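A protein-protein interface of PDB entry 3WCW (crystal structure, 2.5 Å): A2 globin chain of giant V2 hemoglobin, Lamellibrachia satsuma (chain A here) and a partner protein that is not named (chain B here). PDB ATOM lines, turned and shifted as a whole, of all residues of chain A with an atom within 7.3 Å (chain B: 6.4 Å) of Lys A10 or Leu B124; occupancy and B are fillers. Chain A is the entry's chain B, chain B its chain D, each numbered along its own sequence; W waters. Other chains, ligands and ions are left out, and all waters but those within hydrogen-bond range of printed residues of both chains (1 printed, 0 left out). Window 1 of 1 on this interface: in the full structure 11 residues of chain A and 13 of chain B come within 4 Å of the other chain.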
ATOM      1  N   GLY A   4      24.951   3.014   7.243  1.00  0.00           N
ATOM      2  CA  GLY A   4      25.988   3.272   8.226  1.00  0.00           C
ATOM      3  C   GLY A   4      26.677   2.025   8.764  1.00  0.00           C
ATOM      4  O   GLY A   4      26.392   0.912   8.318  1.00  0.00           O
ATOM      5  N   PRO A   5      27.594   2.183   9.731  1.00  0.00           N
ATOM      6  CA  PRO A   5      28.333   1.067  10.338  1.00  0.00           C
ATOM      7  C   PRO A   5      27.389   0.053  10.971  1.00  0.00           C
ATOM      8  O   PRO A   5      27.523  -1.156  10.772  1.00  0.00           O
ATOM      9  CB  PRO A   5      29.205   1.753  11.387  1.00  0.00           C
ATOM     10  CG  PRO A   5      29.398   3.134  10.827  1.00  0.00           C
ATOM     11  CD  PRO A   5      28.020   3.468  10.310  1.00  0.00           C
ATOM     12  N   LEU A   6      26.435   0.559  11.747  1.00  0.00           N
ATOM     13  CA  LEU A   6      25.465  -0.300  12.400  1.00  0.00           C
ATOM     14  C   LEU A   6      24.639  -1.050  11.348  1.00  0.00           C
ATOM     15  O   LEU A   6      24.569  -2.277  11.386  1.00  0.00           O
ATOM     16  CB  LEU A   6      24.559   0.533  13.319  1.00  0.00           C
ATOM     17  CG  LEU A   6      25.262   1.241  14.489  1.00  0.00           C
ATOM     18  CD1 LEU A   6      24.273   2.148  15.214  1.00  0.00           C
ATOM     19  CD2 LEU A   6      25.844   0.209  15.453  1.00  0.00           C
ATOM     20  N   GLN A   7      24.034  -0.322  10.409  1.00  0.00           N
ATOM     21  CA  GLN A   7      23.234  -0.948   9.357  1.00  0.00           C
ATOM     22  C   GLN A   7      24.024  -2.052   8.661  1.00  0.00           C
ATOM     23  O   GLN A   7      23.463  -3.082   8.275  1.00  0.00           O
ATOM     24  CB  GLN A   7      22.801   0.072   8.298  1.00  0.00           C
ATOM     25  CG  GLN A   7      21.679   1.009   8.704  1.00  0.00           C
ATOM     26  CD  GLN A   7      22.057   1.919   9.857  1.00  0.00           C
ATOM     27  OE1 GLN A   7      23.195   2.377   9.961  1.00  0.00           O
ATOM     28  NE2 GLN A   7      21.097   2.197  10.721  1.00  0.00           N
ATOM     29  N   ARG A   8      25.324  -1.834   8.500  1.00  0.00           N
ATOM     30  CA  ARG A   8      26.180  -2.816   7.843  1.00  0.00           C
ATOM     31  C   ARG A   8      26.349  -4.106   8.656  1.00  0.00           C
ATOM     32  O   ARG A   8      26.356  -5.208   8.101  1.00  0.00           O
ATOM     33  CB  ARG A   8      27.541  -2.194   7.532  1.00  0.00           C
ATOM     34  CG  ARG A   8      27.451  -1.165   6.436  1.00  0.00           C
ATOM     35  CD  ARG A   8      28.704  -0.315   6.318  1.00  0.00           C
ATOM     36  NE  ARG A   8      28.438   0.815   5.437  1.00  0.00           N
ATOM     37  CZ  ARG A   8      28.923   0.960   4.208  1.00  0.00           C
ATOM     38  NH1 ARG A   8      29.739   0.040   3.688  1.00  0.00           N
ATOM     39  NH2 ARG A   8      28.554   2.017   3.486  1.00  0.00           N
ATOM     40  N   LEU A   9      26.494  -3.968   9.968  1.00  0.00           N
ATOM     41  CA  LEU A   9      26.626  -5.140  10.815  1.00  0.00           C
ATOM     42  C   LEU A   9      25.315  -5.929  10.732  1.00  0.00           C
ATOM     43  O   LEU A   9      25.323  -7.161  10.665  1.00  0.00           O
ATOM     44  CB  LEU A   9      26.902  -4.726  12.265  1.00  0.00           C
ATOM     45  CG  LEU A   9      28.286  -4.142  12.588  1.00  0.00           C
ATOM     46  CD1 LEU A   9      28.328  -3.756  14.062  1.00  0.00           C
ATOM     47  CD2 LEU A   9      29.390  -5.157  12.281  1.00  0.00           C
ATOM     48  N   LYS A  10      24.196  -5.204  10.703  1.00  0.00           N
ATOM     49  CA  LYS A  10      22.868  -5.807  10.637  1.00  0.00           C
ATOM     50  C   LYS A  10      22.718  -6.634   9.375  1.00  0.00           C
ATOM     51  O   LYS A  10      22.389  -7.823   9.431  1.00  0.00           O
ATOM     52  CB  LYS A  10      21.793  -4.724  10.652  1.00  0.00           C
ATOM     53  CG  LYS A  10      20.375  -5.246  10.857  1.00  0.00           C
ATOM     54  CD  LYS A  10      20.000  -5.285  12.338  1.00  0.00           C
ATOM     55  CE  LYS A  10      18.488  -5.327  12.505  1.00  0.00           C
ATOM     56  NZ  LYS A  10      18.016  -5.017  13.897  1.00  0.00           N
ATOM     57  N   VAL A  11      22.961  -5.987   8.242  1.00  0.00           N
ATOM     58  CA  VAL A  11      22.865  -6.623   6.943  1.00  0.00           C
ATOM     59  C   VAL A  11      23.745  -7.869   6.882  1.00  0.00           C
ATOM     60  O   VAL A  11      23.339  -8.908   6.348  1.00  0.00           O
ATOM     61  CB  VAL A  11      23.254  -5.609   5.818  1.00  0.00           C
ATOM     62  CG1 VAL A  11      23.462  -6.320   4.494  1.00  0.00           C
ATOM     63  CG2 VAL A  11      22.139  -4.580   5.651  1.00  0.00           C
ATOM     64  N   LYS A  12      24.945  -7.773   7.439  1.00  0.00           N
ATOM     65  CA  LYS A  12      25.860  -8.896   7.435  1.00  0.00           C
ATOM     66  C   LYS A  12      25.263 -10.123   8.101  1.00  0.00           C
ATOM     67  O   LYS A  12      25.238 -11.203   7.517  1.00  0.00           O
ATOM     68  CB  LYS A  12      27.174  -8.513   8.128  1.00  0.00           C
ATOM     69  CG  LYS A  12      28.195  -7.883   7.191  1.00  0.00           C
ATOM     70  CD  LYS A  12      29.307  -7.189   7.957  1.00  0.00           C
ATOM     71  CE  LYS A  12      30.521  -6.915   7.074  1.00  0.00           C
ATOM     72  NZ  LYS A  12      31.374  -8.130   6.911  1.00  0.00           N
ATOM     73  N   ARG A  13      24.780  -9.946   9.324  1.00  0.00           N
ATOM     74  CA  ARG A  13      24.189 -11.032  10.097  1.00  0.00           C
ATOM     75  C   ARG A  13      22.911 -11.555   9.439  1.00  0.00           C
ATOM     76  O   ARG A  13      22.746 -12.759   9.284  1.00  0.00           O
ATOM     77  CB  ARG A  13      23.914 -10.553  11.528  1.00  0.00           C
ATOM     78  CG  ARG A  13      23.502 -11.646  12.500  1.00  0.00           C
ATOM     79  CD  ARG A  13      23.393 -11.094  13.914  1.00  0.00           C
ATOM     80  NE  ARG A  13      22.505  -9.932  14.004  1.00  0.00           N
ATOM     81  CZ  ARG A  13      21.182  -9.980  13.879  1.00  0.00           C
ATOM     82  NH1 ARG A  13      20.471  -8.868  13.973  1.00  0.00           N
ATOM     83  NH2 ARG A  13      20.564 -11.135  13.678  1.00  0.00           N
ATOM     84  N   GLN A  14      22.009 -10.662   9.045  1.00  0.00           N
ATOM     85  CA  GLN A  14      20.792 -11.110   8.390  1.00  0.00           C
ATOM     86  C   GLN A  14      21.136 -11.911   7.132  1.00  0.00           C
ATOM     87  O   GLN A  14      20.534 -12.966   6.885  1.00  0.00           O
ATOM     88  CB  GLN A  14      19.891  -9.927   8.050  1.00  0.00           C
ATOM     89  CG  GLN A  14      19.400  -9.194   9.291  1.00  0.00           C
ATOM     90  CD  GLN A  14      18.030  -8.566   9.100  1.00  0.00           C
ATOM     91  OE1 GLN A  14      17.789  -7.859   8.123  1.00  0.00           O
ATOM     92  NE2 GLN A  14      17.126  -8.816  10.042  1.00  0.00           N
ATOM     93  N   TRP A  15      22.108 -11.423   6.354  1.00  0.00           N
ATOM     94  CA  TRP A  15      22.547 -12.115   5.135  1.00  0.00           C
ATOM     95  C   TRP A  15      23.114 -13.485   5.465  1.00  0.00           C
ATOM     96  O   TRP A  15      22.821 -14.462   4.777  1.00  0.00           O
ATOM     97  CB  TRP A  15      23.613 -11.306   4.384  1.00  0.00           C
ATOM     98  CG  TRP A  15      24.258 -12.086   3.251  1.00  0.00           C
ATOM     99  CD1 TRP A  15      25.490 -12.690   3.260  1.00  0.00           C
ATOM    100  CD2 TRP A  15      23.690 -12.360   1.958  1.00  0.00           C
ATOM    101  NE1 TRP A  15      25.725 -13.319   2.051  1.00  0.00           N
ATOM    102  CE2 TRP A  15      24.635 -13.130   1.237  1.00  0.00           C
ATOM    103  CE3 TRP A  15      22.477 -12.027   1.338  1.00  0.00           C
ATOM    104  CZ2 TRP A  15      24.400 -13.570  -0.072  1.00  0.00           C
ATOM    105  CZ3 TRP A  15      22.247 -12.467   0.030  1.00  0.00           C
ATOM    106  CH2 TRP A  15      23.202 -13.228  -0.653  1.00  0.00           C
ATOM    107  N   ALA A  16      23.933 -13.557   6.510  1.00  0.00           N
ATOM    108  CA  ALA A  16      24.517 -14.835   6.919  1.00  0.00           C
ATOM    109  C   ALA A  16      23.417 -15.868   7.149  1.00  0.00           C
ATOM    110  O   ALA A  16      23.542 -17.007   6.722  1.00  0.00           O
ATOM    111  CB  ALA A  16      25.345 -14.668   8.179  1.00  0.00           C
ATOM    112  N   VAL A  75      28.604  -8.032   0.692  1.00  0.00           N
ATOM    113  CA  VAL A  75      28.114  -7.912   2.062  1.00  0.00           C
ATOM    114  C   VAL A  75      29.257  -8.200   3.044  1.00  0.00           C
ATOM    115  O   VAL A  75      29.414  -7.511   4.057  1.00  0.00           O
ATOM    116  CB  VAL A  75      26.930  -8.887   2.342  1.00  0.00           C
ATOM    117  CG1 VAL A  75      26.456  -8.723   3.773  1.00  0.00           C
ATOM    118  CG2 VAL A  75      25.785  -8.610   1.379  1.00  0.00           C
ATOM    119  N   LEU A  78      31.225  -5.049   3.441  1.00  0.00           N
ATOM    120  CA  LEU A  78      30.588  -3.779   3.785  1.00  0.00           C
ATOM    121  C   LEU A  78      31.308  -2.978   4.869  1.00  0.00           C
ATOM    122  O   LEU A  78      30.949  -1.832   5.127  1.00  0.00           O
ATOM    123  CB  LEU A  78      29.129  -3.993   4.206  1.00  0.00           C
ATOM    124  CG  LEU A  78      28.117  -4.370   3.121  1.00  0.00           C
ATOM    125  CD1 LEU A  78      26.718  -4.441   3.730  1.00  0.00           C
ATOM    126  CD2 LEU A  78      28.149  -3.344   2.008  1.00  0.00           C
ATOM    127  N   ILE A 120      14.470 -15.101   6.484  1.00  0.00           N
ATOM    128  CA  ILE A 120      14.582 -14.920   7.931  1.00  0.00           C
ATOM    129  C   ILE A 120      13.288 -14.490   8.615  1.00  0.00           C
ATOM    130  O   ILE A 120      13.226 -14.438   9.848  1.00  0.00           O
ATOM    131  CB  ILE A 120      15.707 -13.912   8.294  1.00  0.00           C
ATOM    132  CG1 ILE A 120      15.453 -12.564   7.616  1.00  0.00           C
ATOM    133  CG2 ILE A 120      17.060 -14.469   7.872  1.00  0.00           C
ATOM    134  CD1 ILE A 120      16.554 -11.558   7.833  1.00  0.00           C
ATOM    135  N   VAL A 124      11.810 -10.137  11.653  1.00  0.00           N
ATOM    136  CA  VAL A 124      13.104  -9.513  11.949  1.00  0.00           C
ATOM    137  C   VAL A 124      13.742  -8.713  10.808  1.00  0.00           C
ATOM    138  O   VAL A 124      14.702  -7.966  11.032  1.00  0.00           O
ATOM    139  CB  VAL A 124      14.142 -10.566  12.432  1.00  0.00           C
ATOM    140  CG1 VAL A 124      13.675 -11.206  13.716  1.00  0.00           C
ATOM    141  CG2 VAL A 124      14.352 -11.615  11.354  1.00  0.00           C
ATOM    142  N   PHE A 125      13.209  -8.865   9.597  1.00  0.00           N
ATOM    143  CA  PHE A 125      13.745  -8.163   8.435  1.00  0.00           C
ATOM    144  C   PHE A 125      13.892  -6.653   8.641  1.00  0.00           C
ATOM    145  O   PHE A 125      12.911  -5.952   8.884  1.00  0.00           O
ATOM    146  CB  PHE A 125      12.866  -8.419   7.218  1.00  0.00           C
ATOM    147  CG  PHE A 125      13.444  -7.882   5.944  1.00  0.00           C
ATOM    148  CD1 PHE A 125      14.710  -8.285   5.518  1.00  0.00           C
ATOM    149  CD2 PHE A 125      12.726  -6.985   5.162  1.00  0.00           C
ATOM    150  CE1 PHE A 125      15.255  -7.799   4.326  1.00  0.00           C
ATOM    151  CE2 PHE A 125      13.260  -6.493   3.967  1.00  0.00           C
ATOM    152  CZ  PHE A 125      14.529  -6.903   3.550  1.00  0.00           C
ATOM    153  N   ASP A 126      15.129  -6.163   8.553  1.00  0.00           N
ATOM    154  CA  ASP A 126      15.416  -4.738   8.731  1.00  0.00           C
ATOM    155  C   ASP A 126      15.414  -4.044   7.347  1.00  0.00           C
ATOM    156  O   ASP A 126      16.440  -3.921   6.673  1.00  0.00           O
ATOM    157  CB  ASP A 126      16.765  -4.572   9.467  1.00  0.00           C
ATOM    158  CG  ASP A 126      17.015  -3.138   9.952  1.00  0.00           C
ATOM    159  OD1 ASP A 126      17.852  -2.945  10.872  1.00  0.00           O
ATOM    160  OD2 ASP A 126      16.390  -2.200   9.410  1.00  0.00           O
ATOM    161  N   LYS A 127      14.226  -3.614   6.942  1.00  0.00           N
ATOM    162  CA  LYS A 127      13.988  -2.961   5.658  1.00  0.00           C
ATOM    163  C   LYS A 127      14.922  -1.793   5.352  1.00  0.00           C
ATOM    164  O   LYS A 127      15.567  -1.774   4.307  1.00  0.00           O
ATOM    165  CB  LYS A 127      12.530  -2.489   5.599  1.00  0.00           C
ATOM    166  CG  LYS A 127      12.148  -1.678   4.362  1.00  0.00           C
ATOM    167  CD  LYS A 127      12.014  -2.543   3.133  1.00  0.00           C
ATOM    168  CE  LYS A 127      11.426  -1.748   1.966  1.00  0.00           C
ATOM    169  NZ  LYS A 127      10.101  -1.145   2.303  1.00  0.00           N
ATOM    170  N   ALA A 129      17.871  -0.818   6.744  1.00  0.00           N
ATOM    171  CA  ALA A 129      19.262  -1.215   6.616  1.00  0.00           C
ATOM    172  C   ALA A 129      19.499  -1.904   5.267  1.00  0.00           C
ATOM    173  O   ALA A 129      20.444  -1.580   4.544  1.00  0.00           O
ATOM    174  CB  ALA A 129      19.643  -2.145   7.755  1.00  0.00           C
ATOM    175  N   TRP A 130      18.629  -2.838   4.913  1.00  0.00           N
ATOM    176  CA  TRP A 130      18.815  -3.553   3.661  1.00  0.00           C
ATOM    177  C   TRP A 130      18.712  -2.707   2.400  1.00  0.00           C
ATOM    178  O   TRP A 130      19.504  -2.865   1.474  1.00  0.00           O
ATOM    179  CB  TRP A 130      17.845  -4.736   3.571  1.00  0.00           C
ATOM    180  CG  TRP A 130      18.422  -5.995   4.150  1.00  0.00           C
ATOM    181  CD1 TRP A 130      18.194  -6.510   5.395  1.00  0.00           C
ATOM    182  CD2 TRP A 130      19.352  -6.880   3.513  1.00  0.00           C
ATOM    183  NE1 TRP A 130      18.922  -7.659   5.566  1.00  0.00           N
ATOM    184  CE2 TRP A 130      19.642  -7.909   4.428  1.00  0.00           C
ATOM    185  CE3 TRP A 130      19.970  -6.898   2.257  1.00  0.00           C
ATOM    186  CZ2 TRP A 130      20.524  -8.951   4.129  1.00  0.00           C
ATOM    187  CZ3 TRP A 130      20.850  -7.938   1.959  1.00  0.00           C
ATOM    188  CH2 TRP A 130      21.118  -8.949   2.893  1.00  0.00           C
ATOM    189  N   GLN B  18      23.457 -12.421  20.244  1.00  0.00           N
ATOM    190  CA  GLN B  18      23.152 -12.328  18.827  1.00  0.00           C
ATOM    191  C   GLN B  18      24.159 -11.398  18.134  1.00  0.00           C
ATOM    192  O   GLN B  18      24.557 -11.647  17.004  1.00  0.00           O
ATOM    193  CB  GLN B  18      21.723 -11.797  18.682  1.00  0.00           C
ATOM    194  CG  GLN B  18      21.140 -11.744  17.295  1.00  0.00           C
ATOM    195  CD  GLN B  18      19.748 -11.139  17.324  1.00  0.00           C
ATOM    196  OE1 GLN B  18      19.379 -10.360  16.447  1.00  0.00           O
ATOM    197  NE2 GLN B  18      18.968 -11.492  18.345  1.00  0.00           N
ATOM    198  N   ILE B  19      24.584 -10.337  18.815  1.00  0.00           N
ATOM    199  CA  ILE B  19      25.549  -9.394  18.231  1.00  0.00           C
ATOM    200  C   ILE B  19      26.913  -9.393  18.914  1.00  0.00           C
ATOM    201  O   ILE B  19      27.841  -8.742  18.444  1.00  0.00           O
ATOM    202  CB  ILE B  19      25.036  -7.949  18.269  1.00  0.00           C
ATOM    203  CG1 ILE B  19      24.641  -7.581  19.701  1.00  0.00           C
ATOM    204  CG2 ILE B  19      23.871  -7.790  17.320  1.00  0.00           C
ATOM    205  CD1 ILE B  19      24.587  -6.101  19.960  1.00  0.00           C
ATOM    206  N   MET B  32      30.971  -1.091  17.038  1.00  0.00           N
ATOM    207  CA  MET B  32      29.861  -0.847  17.951  1.00  0.00           C
ATOM    208  C   MET B  32      30.355   0.099  19.043  1.00  0.00           C
ATOM    209  O   MET B  32      29.625   0.990  19.488  1.00  0.00           O
ATOM    210  CB  MET B  32      29.378  -2.161  18.583  1.00  0.00           C
ATOM    211  CG  MET B  32      28.733  -3.130  17.600  1.00  0.00           C
ATOM    212  SD  MET B  32      28.541  -4.777  18.316  1.00  0.00           S
ATOM    213  CE  MET B  32      27.301  -4.439  19.512  1.00  0.00           C
ATOM    214  N   VAL B 120      21.046   2.666  20.189  1.00  0.00           N
ATOM    215  CA  VAL B 120      21.880   1.917  19.256  1.00  0.00           C
ATOM    216  C   VAL B 120      21.554   0.428  19.128  1.00  0.00           C
ATOM    217  O   VAL B 120      21.464  -0.092  18.013  1.00  0.00           O
ATOM    218  CB  VAL B 120      23.372   2.031  19.639  1.00  0.00           C
ATOM    219  CG1 VAL B 120      24.239   1.397  18.559  1.00  0.00           C
ATOM    220  CG2 VAL B 120      23.751   3.484  19.843  1.00  0.00           C
ATOM    221  N   LEU B 121      21.394  -0.263  20.258  1.00  0.00           N
ATOM    222  CA  LEU B 121      21.094  -1.695  20.226  1.00  0.00           C
ATOM    223  C   LEU B 121      19.948  -2.093  19.273  1.00  0.00           C
ATOM    224  O   LEU B 121      20.057  -3.096  18.552  1.00  0.00           O
ATOM    225  CB  LEU B 121      20.837  -2.217  21.647  1.00  0.00           C
ATOM    226  CG  LEU B 121      22.074  -2.169  22.560  1.00  0.00           C
ATOM    227  CD1 LEU B 121      21.727  -2.715  23.921  1.00  0.00           C
ATOM    228  CD2 LEU B 121      23.216  -2.986  21.953  1.00  0.00           C
ATOM    229  N   PRO B 122      18.844  -1.319  19.248  1.00  0.00           N
ATOM    230  CA  PRO B 122      17.755  -1.690  18.338  1.00  0.00           C
ATOM    231  C   PRO B 122      18.180  -1.694  16.874  1.00  0.00           C
ATOM    232  O   PRO B 122      17.650  -2.454  16.068  1.00  0.00           O
ATOM    233  CB  PRO B 122      16.663  -0.657  18.645  1.00  0.00           C
ATOM    234  CG  PRO B 122      17.411   0.483  19.232  1.00  0.00           C
ATOM    235  CD  PRO B 122      18.443  -0.186  20.097  1.00  0.00           C
ATOM    236  N   SER B 123      19.142  -0.850  16.522  1.00  0.00           N
ATOM    237  CA  SER B 123      19.609  -0.826  15.138  1.00  0.00           C
ATOM    238  C   SER B 123      20.405  -2.089  14.863  1.00  0.00           C
ATOM    239  O   SER B 123      20.553  -2.490  13.716  1.00  0.00           O
ATOM    240  CB  SER B 123      20.515   0.378  14.876  1.00  0.00           C
ATOM    241  OG  SER B 123      19.899   1.583  15.282  1.00  0.00           O
ATOM    242  N   LEU B 124      20.911  -2.713  15.924  1.00  0.00           N
ATOM    243  CA  LEU B 124      21.740  -3.912  15.796  1.00  0.00           C
ATOM    244  C   LEU B 124      21.056  -5.248  16.037  1.00  0.00           C
ATOM    245  O   LEU B 124      21.347  -6.232  15.359  1.00  0.00           O
ATOM    246  CB  LEU B 124      22.937  -3.819  16.750  1.00  0.00           C
ATOM    247  CG  LEU B 124      24.072  -2.863  16.404  1.00  0.00           C
ATOM    248  CD1 LEU B 124      25.005  -2.728  17.589  1.00  0.00           C
ATOM    249  CD2 LEU B 124      24.805  -3.383  15.178  1.00  0.00           C
ATOM    250  N   ILE B 125      20.162  -5.281  17.016  1.00  0.00           N
ATOM    251  CA  ILE B 125      19.471  -6.502  17.399  1.00  0.00           C
ATOM    252  C   ILE B 125      18.100  -6.729  16.740  1.00  0.00           C
ATOM    253  O   ILE B 125      17.347  -5.777  16.494  1.00  0.00           O
ATOM    254  CB  ILE B 125      19.333  -6.527  18.948  1.00  0.00           C
ATOM    255  CG1 ILE B 125      20.734  -6.501  19.580  1.00  0.00           C
ATOM    256  CG2 ILE B 125      18.565  -7.751  19.410  1.00  0.00           C
ATOM    257  CD1 ILE B 125      20.742  -6.229  21.079  1.00  0.00           C
ATOM    258  N   ASP B 126      17.802  -8.001  16.451  1.00  0.00           N
ATOM    259  CA  ASP B 126      16.533  -8.416  15.859  1.00  0.00           C
ATOM    260  C   ASP B 126      15.456  -8.450  16.937  1.00  0.00           C
ATOM    261  O   ASP B 126      15.598  -9.157  17.951  1.00  0.00           O
ATOM    262  CB  ASP B 126      16.641  -9.821  15.260  1.00  0.00           C
ATOM    263  CG  ASP B 126      17.442  -9.857  13.987  1.00  0.00           C
ATOM    264  OD1 ASP B 126      17.777  -8.779  13.459  1.00  0.00           O
ATOM    265  OD2 ASP B 126      17.733 -10.971  13.505  1.00  0.00           O
ATOM    266  N   ASN B 127      14.375  -7.704  16.711  1.00  0.00           N
ATOM    267  CA  ASN B 127      13.264  -7.637  17.660  1.00  0.00           C
ATOM    268  C   ASN B 127      13.700  -7.192  19.028  1.00  0.00           C
ATOM    269  O   ASN B 127      13.295  -7.768  20.032  1.00  0.00           O
ATOM    270  CB  ASN B 127      12.569  -8.989  17.797  1.00  0.00           C
ATOM    271  CG  ASN B 127      11.437  -9.155  16.813  1.00  0.00           C
ATOM    272  OD1 ASN B 127      10.443  -8.413  16.852  1.00  0.00           O
ATOM    273  ND2 ASN B 127      11.576 -10.131  15.918  1.00  0.00           N
ATOM    274  N   PHE B 128      14.532  -6.164  19.059  1.00  0.00           N
ATOM    275  CA  PHE B 128      15.039  -5.606  20.300  1.00  0.00           C
ATOM    276  C   PHE B 128      13.903  -5.424  21.292  1.00  0.00           C
ATOM    277  O   PHE B 128      12.861  -4.870  20.938  1.00  0.00           O
ATOM    278  CB  PHE B 128      15.678  -4.245  20.019  1.00  0.00           C
ATOM    279  CG  PHE B 128      16.142  -3.527  21.253  1.00  0.00           C
ATOM    280  CD1 PHE B 128      17.243  -3.991  21.971  1.00  0.00           C
ATOM    281  CD2 PHE B 128      15.483  -2.378  21.694  1.00  0.00           C
ATOM    282  CE1 PHE B 128      17.681  -3.328  23.098  1.00  0.00           C
ATOM    283  CE2 PHE B 128      15.922  -1.705  22.826  1.00  0.00           C
ATOM    284  CZ  PHE B 128      17.026  -2.183  23.531  1.00  0.00           C
HETATM  285  O   HOH W   1      19.943  -1.282  11.327  1.00  0.00           O
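The backbone carbonyl oxygen of Pro B122 lies within hydrogen-bond range of the side-chain amino group of Lys A10.
The side-chain amino group of Lys A10 lies within hydrogen-bond range of the backbone carbonyl oxygen of Ile B125.
The side-chain amino group (NZ) of Lys A10 lies within salt-bridge range of the side-chain carboxylate (OD1) of Asp B126 (3.8 Å).
The side-chain amide oxygen of Gln B18 lies within hydrogen-bond range of the guanidinium group of Arg A13, at 3.1 Å.
The guanidinium group (NH1) of Arg A13 is in hydrogen-bond range of the backbone carbonyl oxygen (O) of Leu B124, 3.1 Å away.
The guanidinium group (NH1) of Arg A13 lies within salt-bridge range of the side-chain carboxylate (OD1) of Asp B126 (2.7 Å).
The side-chain carboxylate of Asp B126 sits at hydrogen-bond distance from the side-chain amide nitrogen of Gln A14 (3.5 Å).
The side-chain amino group (NZ) of Lys A10 is in salt-bridge range of the side-chain carboxylate (OD1) of Asp A126 (3.7 Å).
The side-chain amide nitrogen (NE2) of Gln A14 is in hydrogen-bond range of the backbone carbonyl oxygen (O) of Val A124.
The side-chain amide oxygen of Gln A14 is in hydrogen-bond range of the backbone NH of Asp A126 (3.2 Å).
OE1 of Gln A14 sits at hydrogen-bond distance from NE1 of Trp A130 (2.8 Å).
The backbone NH of Ala A129 is in hydrogen-bond range of the side-chain carboxylate of Asp A126, 3.3 Å away.
The side-chain amide oxygen (OE1) of Gln B18 is in hydrogen-bond range of the backbone NH (N) of Asp B126 (2.8 Å).
Among the printed residues, merely in contact across the chains: Leu A6 with Val B120 (3.4 Å), Leu A6 with Leu B124 (3.7 Å), Leu A9 with Met B32 (3.6 Å), Leu A9 with Leu B124 (3.7 Å), Lys A10 with Ser B123 (3.2 Å), Lys A10 with Leu B124 (3.4 Å), Val A124 with Asp B126 (3.6 Å), Val A124 with Asn B127 (3.2 Å) and Asp A126 with Ser B123 (3.9 Å).
Gly A4 touches none of the printed residues of chain B.
Of the printed residues of chain B, Leu A6 touches Val B120 (3.4 Å) and Leu B124 (3.7 Å).
Of chain B, only Pro B122, Ser B123, Leu B124, Ile B125 and Asp B126 come within 4 Å of Lys A10.
Printed residues of chain B within 4 Å of Val A124: Asp B126 (3.6 Å) and Asn B127 (3.2 Å).
Printed residues of chain A within 4 Å of Val B120: Leu A6.
Of the printed residues of chain A, Pro B122 touches Lys A10.
Of chain A, only Leu A6 (3.7 Å), Leu A9 (3.7 Å), Lys A10 (3.4 Å) and Arg A13 (3.1 Å) come within 4 Å of Leu B124.
Phe B128 touches none of the printed residues of chain A.
The nearest residue of chain B that does not touch Lys A10 is Asn B127 (5.3 Å).
The nearest residue of chain A that does not touch Leu B124 is Pro A5 (5.6 Å).
Of the 12 printed residues of chain B, 9 touch a printed residue of chain A.
Hydrophobic or aromatic side chains of chain B within 4 Å of the printed part of chain A: Met B32, Val B120 and Leu B124.
Of the 22 printed residues of chain A, 7 touch a printed residue of chain B.
Hydrophobic or aromatic side chains of chain A within 4 Å of the printed part of chain B: Leu A6, Leu A9 and Val A124.
Among the printed residues, Asp or Glu carboxylates within 4 Å of a Lys or Arg side-chain nitrogen of the other chain: Lys A10 with Asp B126 (3.8 Å) and Arg A13 with Asp B126 (2.7 Å).
Water W1 lies within hydrogen-bond range of the side-chain carboxylate (OD1) of Asp A126 (2.7 Å) and the backbone carbonyl oxygen (O) of Ser B123 (2.7 Å).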
